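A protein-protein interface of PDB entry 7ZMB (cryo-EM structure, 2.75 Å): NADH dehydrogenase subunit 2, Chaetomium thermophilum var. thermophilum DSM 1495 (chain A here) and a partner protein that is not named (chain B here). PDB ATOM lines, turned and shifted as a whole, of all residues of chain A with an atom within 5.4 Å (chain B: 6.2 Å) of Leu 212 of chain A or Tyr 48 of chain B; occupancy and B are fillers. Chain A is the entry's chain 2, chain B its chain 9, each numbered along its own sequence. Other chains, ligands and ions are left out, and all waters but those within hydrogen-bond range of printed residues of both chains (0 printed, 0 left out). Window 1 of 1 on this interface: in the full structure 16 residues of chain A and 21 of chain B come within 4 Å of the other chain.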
ATOM      1  N   ASN A 200      32.067 -11.252  32.637  1.00  0.00           N
ATOM      2  CA  ASN A 200      30.975 -10.539  31.990  1.00  0.00           C
ATOM      3  C   ASN A 200      30.712 -11.008  30.571  1.00  0.00           C
ATOM      4  O   ASN A 200      29.597 -10.833  30.081  1.00  0.00           O
ATOM      5  CB  ASN A 200      31.251  -9.040  31.979  1.00  0.00           C
ATOM      6  CG  ASN A 200      31.259  -8.442  33.354  1.00  0.00           C
ATOM      7  OD1 ASN A 200      30.236  -8.383  34.014  1.00  0.00           O
ATOM      8  ND2 ASN A 200      32.418  -8.006  33.804  1.00  0.00           N
ATOM      9  N   SER A 201      31.717 -11.610  29.930  1.00  0.00           N
ATOM     10  CA  SER A 201      31.575 -11.969  28.491  1.00  0.00           C
ATOM     11  C   SER A 201      31.495 -13.474  28.236  1.00  0.00           C
ATOM     12  O   SER A 201      31.191 -13.812  27.091  1.00  0.00           O
ATOM     13  CB  SER A 201      32.749 -11.426  27.742  1.00  0.00           C
ATOM     14  OG  SER A 201      33.934 -12.114  28.096  1.00  0.00           O
ATOM     15  N   THR A 203      33.827 -15.576  27.770  1.00  0.00           N
ATOM     16  CA  THR A 203      34.864 -16.052  26.825  1.00  0.00           C
ATOM     17  C   THR A 203      36.269 -15.686  27.299  1.00  0.00           C
ATOM     18  O   THR A 203      36.413 -14.644  27.947  1.00  0.00           O
ATOM     19  CB  THR A 203      34.628 -15.497  25.409  1.00  0.00           C
ATOM     20  OG1 THR A 203      35.789 -15.722  24.613  1.00  0.00           O
ATOM     21  CG2 THR A 203      34.298 -14.021  25.378  1.00  0.00           C
ATOM     22  N   GLY A 208      37.113 -13.236  20.479  1.00  0.00           N
ATOM     23  CA  GLY A 208      35.683 -13.106  20.826  1.00  0.00           C
ATOM     24  C   GLY A 208      35.312 -11.760  21.445  1.00  0.00           C
ATOM     25  O   GLY A 208      34.257 -11.235  21.081  1.00  0.00           O
ATOM     26  N   LEU A 209      36.130 -11.214  22.343  1.00  0.00           N
ATOM     27  CA  LEU A 209      35.877  -9.888  22.964  1.00  0.00           C
ATOM     28  C   LEU A 209      35.910  -8.770  21.921  1.00  0.00           C
ATOM     29  O   LEU A 209      35.072  -7.867  22.010  1.00  0.00           O
ATOM     30  CB  LEU A 209      36.926  -9.639  24.046  1.00  0.00           C
ATOM     31  CG  LEU A 209      36.792 -10.488  25.309  1.00  0.00           C
ATOM     32  CD1 LEU A 209      38.142 -10.688  25.978  1.00  0.00           C
ATOM     33  CD2 LEU A 209      35.806  -9.861  26.276  1.00  0.00           C
ATOM     34  N   TYR A 210      36.851  -8.834  20.980  1.00  0.00           N
ATOM     35  CA  TYR A 210      36.941  -7.832  19.889  1.00  0.00           C
ATOM     36  C   TYR A 210      35.668  -7.898  19.049  1.00  0.00           C
ATOM     37  O   TYR A 210      35.176  -6.846  18.642  1.00  0.00           O
ATOM     38  CB  TYR A 210      38.177  -8.066  19.024  1.00  0.00           C
ATOM     39  CG  TYR A 210      39.520  -7.955  19.694  1.00  0.00           C
ATOM     40  CD1 TYR A 210      39.712  -7.152  20.807  1.00  0.00           C
ATOM     41  CD2 TYR A 210      40.613  -8.636  19.189  1.00  0.00           C
ATOM     42  CE1 TYR A 210      40.952  -7.051  21.414  1.00  0.00           C
ATOM     43  CE2 TYR A 210      41.861  -8.538  19.777  1.00  0.00           C
ATOM     44  CZ  TYR A 210      42.030  -7.743  20.895  1.00  0.00           C
ATOM     45  OH  TYR A 210      43.254  -7.645  21.483  1.00  0.00           O
ATOM     46  N   ILE A 211      35.144  -9.095  18.797  1.00  0.00           N
ATOM     47  CA  ILE A 211      33.847  -9.209  18.061  1.00  0.00           C
ATOM     48  C   ILE A 211      32.692  -8.593  18.858  1.00  0.00           C
ATOM     49  O   ILE A 211      31.972  -7.781  18.271  1.00  0.00           O
ATOM     50  CB  ILE A 211      33.571 -10.655  17.603  1.00  0.00           C
ATOM     51  CG1 ILE A 211      34.496 -11.061  16.455  1.00  0.00           C
ATOM     52  CG2 ILE A 211      32.110 -10.842  17.222  1.00  0.00           C
ATOM     53  CD1 ILE A 211      33.905 -12.102  15.548  1.00  0.00           C
ATOM     54  N   LEU A 212      32.541  -8.937  20.140  1.00  0.00           N
ATOM     55  CA  LEU A 212      31.492  -8.318  20.993  1.00  0.00           C
ATOM     56  C   LEU A 212      31.644  -6.793  20.977  1.00  0.00           C
ATOM     57  O   LEU A 212      30.622  -6.107  20.851  1.00  0.00           O
ATOM     58  CB  LEU A 212      31.623  -8.856  22.421  1.00  0.00           C
ATOM     59  CG  LEU A 212      31.305 -10.338  22.611  1.00  0.00           C
ATOM     60  CD1 LEU A 212      31.781 -10.823  23.969  1.00  0.00           C
ATOM     61  CD2 LEU A 212      29.817 -10.594  22.449  1.00  0.00           C
ATOM     62  N   ASN A 213      32.873  -6.290  21.086  1.00  0.00           N
ATOM     63  CA  ASN A 213      33.160  -4.835  21.078  1.00  0.00           C
ATOM     64  C   ASN A 213      32.770  -4.202  19.745  1.00  0.00           C
ATOM     65  O   ASN A 213      32.291  -3.054  19.763  1.00  0.00           O
ATOM     66  CB  ASN A 213      34.650  -4.571  21.300  1.00  0.00           C
ATOM     67  CG  ASN A 213      35.031  -3.119  21.107  1.00  0.00           C
ATOM     68  OD1 ASN A 213      36.061  -2.817  20.512  1.00  0.00           O
ATOM     69  ND2 ASN A 213      34.203  -2.211  21.595  1.00  0.00           N
ATOM     70  N   SER A 214      32.965  -4.903  18.630  1.00  0.00           N
ATOM     71  CA  SER A 214      32.716  -4.267  17.317  1.00  0.00           C
ATOM     72  C   SER A 214      31.209  -4.225  17.066  1.00  0.00           C
ATOM     73  O   SER A 214      30.747  -3.226  16.498  1.00  0.00           O
ATOM     74  CB  SER A 214      33.410  -5.028  16.239  1.00  0.00           C
ATOM     75  OG  SER A 214      33.136  -4.472  14.963  1.00  0.00           O
ATOM     76  N   ILE A 215      30.472  -5.248  17.506  1.00  0.00           N
ATOM     77  CA  ILE A 215      29.023  -5.180  17.361  1.00  0.00           C
ATOM     78  C   ILE A 215      28.465  -4.039  18.190  1.00  0.00           C
ATOM     79  O   ILE A 215      27.621  -3.265  17.723  1.00  0.00           O
ATOM     80  CB  ILE A 215      28.378  -6.522  17.751  1.00  0.00           C
ATOM     81  CG1 ILE A 215      28.962  -7.661  16.925  1.00  0.00           C
ATOM     82  CG2 ILE A 215      26.890  -6.467  17.562  1.00  0.00           C
ATOM     83  CD1 ILE A 215      28.510  -9.007  17.372  1.00  0.00           C
ATOM     84  N   SER A 216      28.906  -3.969  19.442  1.00  0.00           N
ATOM     85  CA  SER A 216      28.395  -2.944  20.378  1.00  0.00           C
ATOM     86  C   SER A 216      28.678  -1.541  19.848  1.00  0.00           C
ATOM     87  O   SER A 216      28.127  -0.583  20.414  1.00  0.00           O
ATOM     88  CB  SER A 216      29.032  -3.144  21.704  1.00  0.00           C
ATOM     89  OG  SER A 216      30.403  -2.788  21.662  1.00  0.00           O
ATOM     90  N   ASP A 217      29.498  -1.422  18.806  1.00  0.00           N
ATOM     91  CA  ASP A 217      29.718  -0.082  18.217  1.00  0.00           C
ATOM     92  C   ASP A 217      28.583   0.144  17.226  1.00  0.00           C
ATOM     93  O   ASP A 217      28.672  -0.362  16.092  1.00  0.00           O
ATOM     94  CB  ASP A 217      31.103   0.039  17.580  1.00  0.00           C
ATOM     95  CG  ASP A 217      31.488   1.468  17.237  1.00  0.00           C
ATOM     96  OD1 ASP A 217      30.934   2.391  17.868  1.00  0.00           O
ATOM     97  OD2 ASP A 217      32.333   1.647  16.338  1.00  0.00           O
ATOM     98  N   TYR A 235      22.224  -4.895  28.463  1.00  0.00           N
ATOM     99  CA  TYR A 235      23.625  -5.322  28.676  1.00  0.00           C
ATOM    100  C   TYR A 235      24.555  -4.372  27.928  1.00  0.00           C
ATOM    101  O   TYR A 235      25.249  -4.822  27.002  1.00  0.00           O
ATOM    102  CB  TYR A 235      23.812  -6.754  28.164  1.00  0.00           C
ATOM    103  CG  TYR A 235      22.998  -7.807  28.870  1.00  0.00           C
ATOM    104  CD1 TYR A 235      23.426  -8.343  30.071  1.00  0.00           C
ATOM    105  CD2 TYR A 235      21.811  -8.277  28.332  1.00  0.00           C
ATOM    106  CE1 TYR A 235      22.693  -9.317  30.724  1.00  0.00           C
ATOM    107  CE2 TYR A 235      21.063  -9.248  28.974  1.00  0.00           C
ATOM    108  CZ  TYR A 235      21.507  -9.769  30.176  1.00  0.00           C
ATOM    109  OH  TYR A 235      20.790 -10.728  30.823  1.00  0.00           O
ATOM    110  N   PRO A 237      27.917  -2.719  27.117  1.00  0.00           N
ATOM    111  CA  PRO A 237      29.183  -3.363  27.425  1.00  0.00           C
ATOM    112  C   PRO A 237      30.149  -2.438  28.171  1.00  0.00           C
ATOM    113  O   PRO A 237      31.264  -2.271  27.727  1.00  0.00           O
ATOM    114  CB  PRO A 237      29.663  -3.699  26.005  1.00  0.00           C
ATOM    115  CG  PRO A 237      29.175  -2.552  25.158  1.00  0.00           C
ATOM    116  CD  PRO A 237      27.871  -2.115  25.786  1.00  0.00           C
ATOM    117  N   TYR A 239      31.709  -3.052  30.770  1.00  0.00           N
ATOM    118  CA  TYR A 239      32.813  -3.861  31.340  1.00  0.00           C
ATOM    119  C   TYR A 239      34.060  -3.804  30.467  1.00  0.00           C
ATOM    120  O   TYR A 239      35.129  -3.794  31.055  1.00  0.00           O
ATOM    121  CB  TYR A 239      32.368  -5.308  31.574  1.00  0.00           C
ATOM    122  CG  TYR A 239      32.076  -6.110  30.333  1.00  0.00           C
ATOM    123  CD1 TYR A 239      30.858  -6.008  29.684  1.00  0.00           C
ATOM    124  CD2 TYR A 239      33.015  -6.987  29.816  1.00  0.00           C
ATOM    125  CE1 TYR A 239      30.587  -6.750  28.546  1.00  0.00           C
ATOM    126  CE2 TYR A 239      32.760  -7.737  28.681  1.00  0.00           C
ATOM    127  CZ  TYR A 239      31.540  -7.618  28.046  1.00  0.00           C
ATOM    128  OH  TYR A 239      31.285  -8.349  26.925  1.00  0.00           O
ATOM    129  N   TRP B  18      26.446 -18.536  21.453  1.00  0.00           N
ATOM    130  CA  TRP B  18      27.756 -17.958  21.057  1.00  0.00           C
ATOM    131  C   TRP B  18      28.047 -18.263  19.588  1.00  0.00           C
ATOM    132  O   TRP B  18      28.467 -17.357  18.871  1.00  0.00           O
ATOM    133  CB  TRP B  18      28.852 -18.469  21.985  1.00  0.00           C
ATOM    134  CG  TRP B  18      30.225 -17.988  21.631  1.00  0.00           C
ATOM    135  CD1 TRP B  18      31.247 -18.725  21.109  1.00  0.00           C
ATOM    136  CD2 TRP B  18      30.725 -16.647  21.762  1.00  0.00           C
ATOM    137  NE1 TRP B  18      32.350 -17.940  20.927  1.00  0.00           N
ATOM    138  CE2 TRP B  18      32.059 -16.660  21.311  1.00  0.00           C
ATOM    139  CE3 TRP B  18      30.183 -15.446  22.230  1.00  0.00           C
ATOM    140  CZ2 TRP B  18      32.856 -15.517  21.314  1.00  0.00           C
ATOM    141  CZ3 TRP B  18      30.967 -14.317  22.230  1.00  0.00           C
ATOM    142  CH2 TRP B  18      32.285 -14.353  21.776  1.00  0.00           C
ATOM    143  N   LEU B  21      26.012 -15.957  17.232  1.00  0.00           N
ATOM    144  CA  LEU B  21      26.589 -14.596  17.163  1.00  0.00           C
ATOM    145  C   LEU B  21      27.846 -14.595  16.291  1.00  0.00           C
ATOM    146  O   LEU B  21      27.995 -13.671  15.474  1.00  0.00           O
ATOM    147  CB  LEU B  21      26.895 -14.134  18.584  1.00  0.00           C
ATOM    148  CG  LEU B  21      27.376 -12.700  18.738  1.00  0.00           C
ATOM    149  CD1 LEU B  21      26.377 -11.745  18.111  1.00  0.00           C
ATOM    150  CD2 LEU B  21      27.582 -12.382  20.205  1.00  0.00           C
ATOM    151  N   VAL B  43      21.148 -10.943  18.200  1.00  0.00           N
ATOM    152  CA  VAL B  43      21.907 -12.156  18.473  1.00  0.00           C
ATOM    153  C   VAL B  43      22.865 -11.934  19.637  1.00  0.00           C
ATOM    154  O   VAL B  43      23.058 -12.821  20.473  1.00  0.00           O
ATOM    155  CB  VAL B  43      22.641 -12.608  17.199  1.00  0.00           C
ATOM    156  CG1 VAL B  43      23.166 -14.006  17.351  1.00  0.00           C
ATOM    157  CG2 VAL B  43      21.712 -12.535  16.018  1.00  0.00           C
ATOM    158  N   MET B  44      23.389 -10.712  19.782  1.00  0.00           N
ATOM    159  CA  MET B  44      24.353 -10.387  20.868  1.00  0.00           C
ATOM    160  C   MET B  44      23.670 -10.260  22.224  1.00  0.00           C
ATOM    161  O   MET B  44      24.245 -10.738  23.208  1.00  0.00           O
ATOM    162  CB  MET B  44      25.170  -9.133  20.563  1.00  0.00           C
ATOM    163  CG  MET B  44      26.432  -9.042  21.405  1.00  0.00           C
ATOM    164  SD  MET B  44      27.392  -7.535  21.178  1.00  0.00           S
ATOM    165  CE  MET B  44      26.137  -6.301  21.509  1.00  0.00           C
ATOM    166  N   GLU B  45      22.482  -9.670  22.259  1.00  0.00           N
ATOM    167  CA  GLU B  45      21.701  -9.523  23.507  1.00  0.00           C
ATOM    168  C   GLU B  45      21.295 -10.904  24.027  1.00  0.00           C
ATOM    169  O   GLU B  45      21.280 -11.090  25.251  1.00  0.00           O
ATOM    170  CB  GLU B  45      20.519  -8.593  23.237  1.00  0.00           C
ATOM    171  CG  GLU B  45      19.750  -8.210  24.487  1.00  0.00           C
ATOM    172  CD  GLU B  45      18.696  -7.133  24.290  1.00  0.00           C
ATOM    173  OE1 GLU B  45      18.656  -6.537  23.193  1.00  0.00           O
ATOM    174  OE2 GLU B  45      17.918  -6.891  25.234  1.00  0.00           O
ATOM    175  N   ASP B  46      20.943 -11.815  23.132  1.00  0.00           N
ATOM    176  CA  ASP B  46      20.513 -13.178  23.525  1.00  0.00           C
ATOM    177  C   ASP B  46      21.668 -13.940  24.177  1.00  0.00           C
ATOM    178  O   ASP B  46      21.406 -14.709  25.104  1.00  0.00           O
ATOM    179  CB  ASP B  46      19.921 -13.930  22.334  1.00  0.00           C
ATOM    180  CG  ASP B  46      18.585 -13.406  21.864  1.00  0.00           C
ATOM    181  OD1 ASP B  46      17.917 -12.730  22.656  1.00  0.00           O
ATOM    182  OD2 ASP B  46      18.230 -13.685  20.708  1.00  0.00           O
ATOM    183  N   TYR B  47      22.884 -13.774  23.657  1.00  0.00           N
ATOM    184  CA  TYR B  47      24.059 -14.450  24.249  1.00  0.00           C
ATOM    185  C   TYR B  47      24.262 -13.920  25.666  1.00  0.00           C
ATOM    186  O   TYR B  47      24.532 -14.720  26.572  1.00  0.00           O
ATOM    187  CB  TYR B  47      25.301 -14.268  23.377  1.00  0.00           C
ATOM    188  CG  TYR B  47      26.565 -14.693  24.078  1.00  0.00           C
ATOM    189  CD1 TYR B  47      26.820 -16.031  24.320  1.00  0.00           C
ATOM    190  CD2 TYR B  47      27.462 -13.758  24.561  1.00  0.00           C
ATOM    191  CE1 TYR B  47      27.955 -16.436  24.998  1.00  0.00           C
ATOM    192  CE2 TYR B  47      28.600 -14.145  25.243  1.00  0.00           C
ATOM    193  CZ  TYR B  47      28.847 -15.488  25.460  1.00  0.00           C
ATOM    194  OH  TYR B  47      29.972 -15.878  26.119  1.00  0.00           O
ATOM    195  N   TYR B  48      24.097 -12.615  25.860  1.00  0.00           N
ATOM    196  CA  TYR B  48      24.210 -12.036  27.217  1.00  0.00           C
ATOM    197  C   TYR B  48      23.040 -12.501  28.097  1.00  0.00           C
ATOM    198  O   TYR B  48      23.248 -12.648  29.304  1.00  0.00           O
ATOM    199  CB  TYR B  48      24.316 -10.514  27.151  1.00  0.00           C
ATOM    200  CG  TYR B  48      25.615  -9.931  26.662  1.00  0.00           C
ATOM    201  CD1 TYR B  48      26.825 -10.241  27.262  1.00  0.00           C
ATOM    202  CD2 TYR B  48      25.622  -9.016  25.627  1.00  0.00           C
ATOM    203  CE1 TYR B  48      28.011  -9.683  26.819  1.00  0.00           C
ATOM    204  CE2 TYR B  48      26.796  -8.447  25.173  1.00  0.00           C
ATOM    205  CZ  TYR B  48      27.995  -8.779  25.771  1.00  0.00           C
ATOM    206  OH  TYR B  48      29.140  -8.206  25.305  1.00  0.00           O
ATOM    207  N   GLU B  49      21.850 -12.688  27.521  1.00  0.00           N
ATOM    208  CA  GLU B  49      20.651 -13.125  28.283  1.00  0.00           C
ATOM    209  C   GLU B  49      20.823 -14.562  28.766  1.00  0.00           C
ATOM    210  O   GLU B  49      20.398 -14.849  29.892  1.00  0.00           O
ATOM    211  CB  GLU B  49      19.351 -12.826  27.534  1.00  0.00           C
ATOM    212  CG  GLU B  49      18.096 -13.227  28.274  1.00  0.00           C
ATOM    213  CD  GLU B  49      17.964 -12.694  29.688  1.00  0.00           C
ATOM    214  OE1 GLU B  49      18.454 -11.591  29.949  1.00  0.00           O
ATOM    215  OE2 GLU B  49      17.369 -13.388  30.523  1.00  0.00           O
ATOM    216  N   CYS B  50      21.470 -15.412  27.967  1.00  0.00           N
ATOM    217  CA  CYS B  50      21.679 -16.831  28.340  1.00  0.00           C
ATOM    218  C   CYS B  50      22.791 -16.853  29.373  1.00  0.00           C
ATOM    219  O   CYS B  50      22.822 -17.755  30.187  1.00  0.00           O
ATOM    220  CB  CYS B  50      22.165 -17.611  27.126  1.00  0.00           C
ATOM    221  SG  CYS B  50      22.741 -19.293  27.462  1.00  0.00           S
ATOM    222  N   LEU B  51      23.590 -15.805  29.445  1.00  0.00           N
ATOM    223  CA  LEU B  51      24.729 -15.754  30.397  1.00  0.00           C
ATOM    224  C   LEU B  51      24.306 -15.178  31.754  1.00  0.00           C
ATOM    225  O   LEU B  51      24.592 -15.832  32.760  1.00  0.00           O
ATOM    226  CB  LEU B  51      25.809 -14.879  29.758  1.00  0.00           C
ATOM    227  CG  LEU B  51      27.235 -15.419  29.768  1.00  0.00           C
ATOM    228  CD1 LEU B  51      27.342 -16.703  28.964  1.00  0.00           C
ATOM    229  CD2 LEU B  51      28.186 -14.375  29.212  1.00  0.00           C
ATOM    230  N   HIS B  52      23.657 -14.009  31.782  1.00  0.00           N
ATOM    231  CA  HIS B  52      23.351 -13.309  33.056  1.00  0.00           C
ATOM    232  C   HIS B  52      21.889 -13.460  33.505  1.00  0.00           C
ATOM    233  O   HIS B  52      21.673 -13.495  34.728  1.00  0.00           O
ATOM    234  CB  HIS B  52      23.869 -11.880  32.909  1.00  0.00           C
ATOM    235  CG  HIS B  52      25.283 -11.862  32.440  1.00  0.00           C
ATOM    236  ND1 HIS B  52      26.275 -12.579  33.079  1.00  0.00           N
ATOM    237  CD2 HIS B  52      25.870 -11.260  31.386  1.00  0.00           C
ATOM    238  CE1 HIS B  52      27.414 -12.404  32.447  1.00  0.00           C
ATOM    239  NE2 HIS B  52      27.192 -11.595  31.411  1.00  0.00           N
ATOM    240  N   HIS B  53      20.927 -13.539  32.572  1.00  0.00           N
ATOM    241  CA  HIS B  53      19.491 -13.776  32.896  1.00  0.00           C
ATOM    242  C   HIS B  53      18.747 -12.533  33.412  1.00  0.00           C
ATOM    243  O   HIS B  53      17.701 -12.738  34.033  1.00  0.00           O
ATOM    244  CB  HIS B  53      19.295 -14.969  33.843  1.00  0.00           C
ATOM    245  CG  HIS B  53      20.027 -16.208  33.462  1.00  0.00           C
ATOM    246  ND1 HIS B  53      19.643 -16.995  32.399  1.00  0.00           N
ATOM    247  CD2 HIS B  53      21.101 -16.809  34.013  1.00  0.00           C
ATOM    248  CE1 HIS B  53      20.459 -18.021  32.303  1.00  0.00           C
ATOM    249  NE2 HIS B  53      21.359 -17.930  33.280  1.00  0.00           N
ATOM    250  N   ARG B  54      19.222 -11.313  33.148  1.00  0.00           N
ATOM    251  CA  ARG B  54      18.576 -10.086  33.700  1.00  0.00           C
ATOM    252  C   ARG B  54      17.152  -9.897  33.168  1.00  0.00           C
ATOM    253  O   ARG B  54      16.295  -9.479  33.956  1.00  0.00           O
ATOM    254  CB  ARG B  54      19.409  -8.837  33.429  1.00  0.00           C
ATOM    255  CG  ARG B  54      20.863  -8.967  33.859  1.00  0.00           C
ATOM    256  CD  ARG B  54      21.608  -7.652  33.945  1.00  0.00           C
ATOM    257  NE  ARG B  54      21.433  -7.003  35.237  1.00  0.00           N
ATOM    258  CZ  ARG B  54      20.614  -5.984  35.469  1.00  0.00           C
ATOM    259  NH1 ARG B  54      20.527  -5.472  36.684  1.00  0.00           N
ATOM    260  NH2 ARG B  54      19.893  -5.476  34.486  1.00  0.00           N
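OE1 of Glu 49 of chain B sits at hydrogen-bond distance from N of Arg 54 of chain B, at 3.3 Å.
The side-chain hydroxyl (OG) of Ser 201 of chain A sits close to the backbone NH (N) of Thr 203 of chain A (3.5 Å).
O of Cys 50 of chain B sits close to NE2 of His 53 of chain B, at 3.4 Å.
A ring nitrogen (ND1) of His 53 of chain B sits close to the backbone carbonyl oxygen of Glu 49 of chain B, at 3.4 Å.
The backbone carbonyl oxygen of Leu 212 of chain A lies within hydrogen-bond range of the side-chain hydroxyl of Ser 216 of chain A, at 3.4 Å.
The side-chain hydroxyl of Tyr 239 of chain A lies within hydrogen-bond range of the side-chain hydroxyl of Tyr 48 of chain B (2.7 Å).
The backbone carbonyl oxygen (O) of Ser 201 of chain A sits at hydrogen-bond distance from the side-chain hydroxyl (OH) of Tyr 47 of chain B, 2.6 Å away.
OH of Tyr 235 of chain A sits at hydrogen-bond distance from N of His 53 of chain B (3.3 Å).
A ring nitrogen (NE2) of His 52 of chain B sits at hydrogen-bond distance from the backbone carbonyl oxygen of Asn 200 of chain A, at 2.9 Å.
The side-chain carboxylate of Glu 49 of chain B lies within hydrogen-bond range of the side-chain hydroxyl of Tyr 235 of chain A.
The side-chain hydroxyl of Tyr 235 of chain A sits at hydrogen-bond distance from the backbone carbonyl oxygen of Tyr 48 of chain B.
The side-chain hydroxyl of Tyr 235 of chain A sits at hydrogen-bond distance from the backbone NH of Arg 54 of chain B, 2.9 Å away.
O of Leu 212 of chain A sits close to SD of Met 44 of chain B.
Of chain B, only Trp 18, Leu 21, Met 44 and Tyr 48 come within 4 Å of Leu 212 of chain A.
Ser 216 of chain A touches none of the printed residues of chain B.
Of the printed residues of chain A, Tyr 47 of chain B touches Ser 201.
Of chain A, only Asn 200 (3.8 Å), Leu 212 (3.8 Å), Tyr 235 (3.5 Å) and Tyr 239 (2.7 Å) come within 4 Å of Tyr 48 of chain B.
Of the printed residues of chain A, Leu 51 of chain B touches Asn 200 (3.9 Å) and Ser 201 (3.6 Å).
Of the printed residues of chain A, His 53 of chain B touches Tyr 235 (3.3 Å).
The nearest residue of chain B that does not touch Leu 212 of chain A is Tyr 47 of chain B (4.5 Å).
The nearest residue of chain A that does not touch Tyr 48 of chain B is Ser 201 of chain A (4.6 Å).
The nearest printed residue of chain B that does not touch Gly 208 of chain A is Leu 21 of chain B (6.8 Å).
Tyr 48 of chain B touches Asn 200 of chain A (CE1 to O, 3.8 Å).
Asn 200 of chain A touches Leu 51 of chain B.
C of Ser 201 of chain A touches CD2 of Leu 51 of chain B, at 3.6 Å.
CA of Gly 208 of chain A touches CH2 of Trp 18 of chain B, 3.7 Å away.
Leu 212 of chain A touches Trp 18 of chain B (CD2 to CZ3, 3.9 Å).
CD2 of Leu 212 of chain A touches CD2 of Leu 21 of chain B, 3.6 Å away.
Tyr 48 of chain B touches Leu 212 of chain A.
CD1 of Leu 21 of chain B touches CD1 of Ile 215 of chain A, at 3.5 Å.
Met 44 of chain B touches Ile 215 of chain A (SD to CB, 3.7 Å).
CE1 of Tyr 235 of chain A touches CB of His 52 of chain B, at 3.6 Å.
Printed residues of chain B that touch a printed residue of chain A: Trp 18, Leu 21, Met 44, Tyr 47, Tyr 48, Glu 49, Leu 51, His 52, His 53 and Arg 54.
Among the printed residues, 18 pairs touch across the chains.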
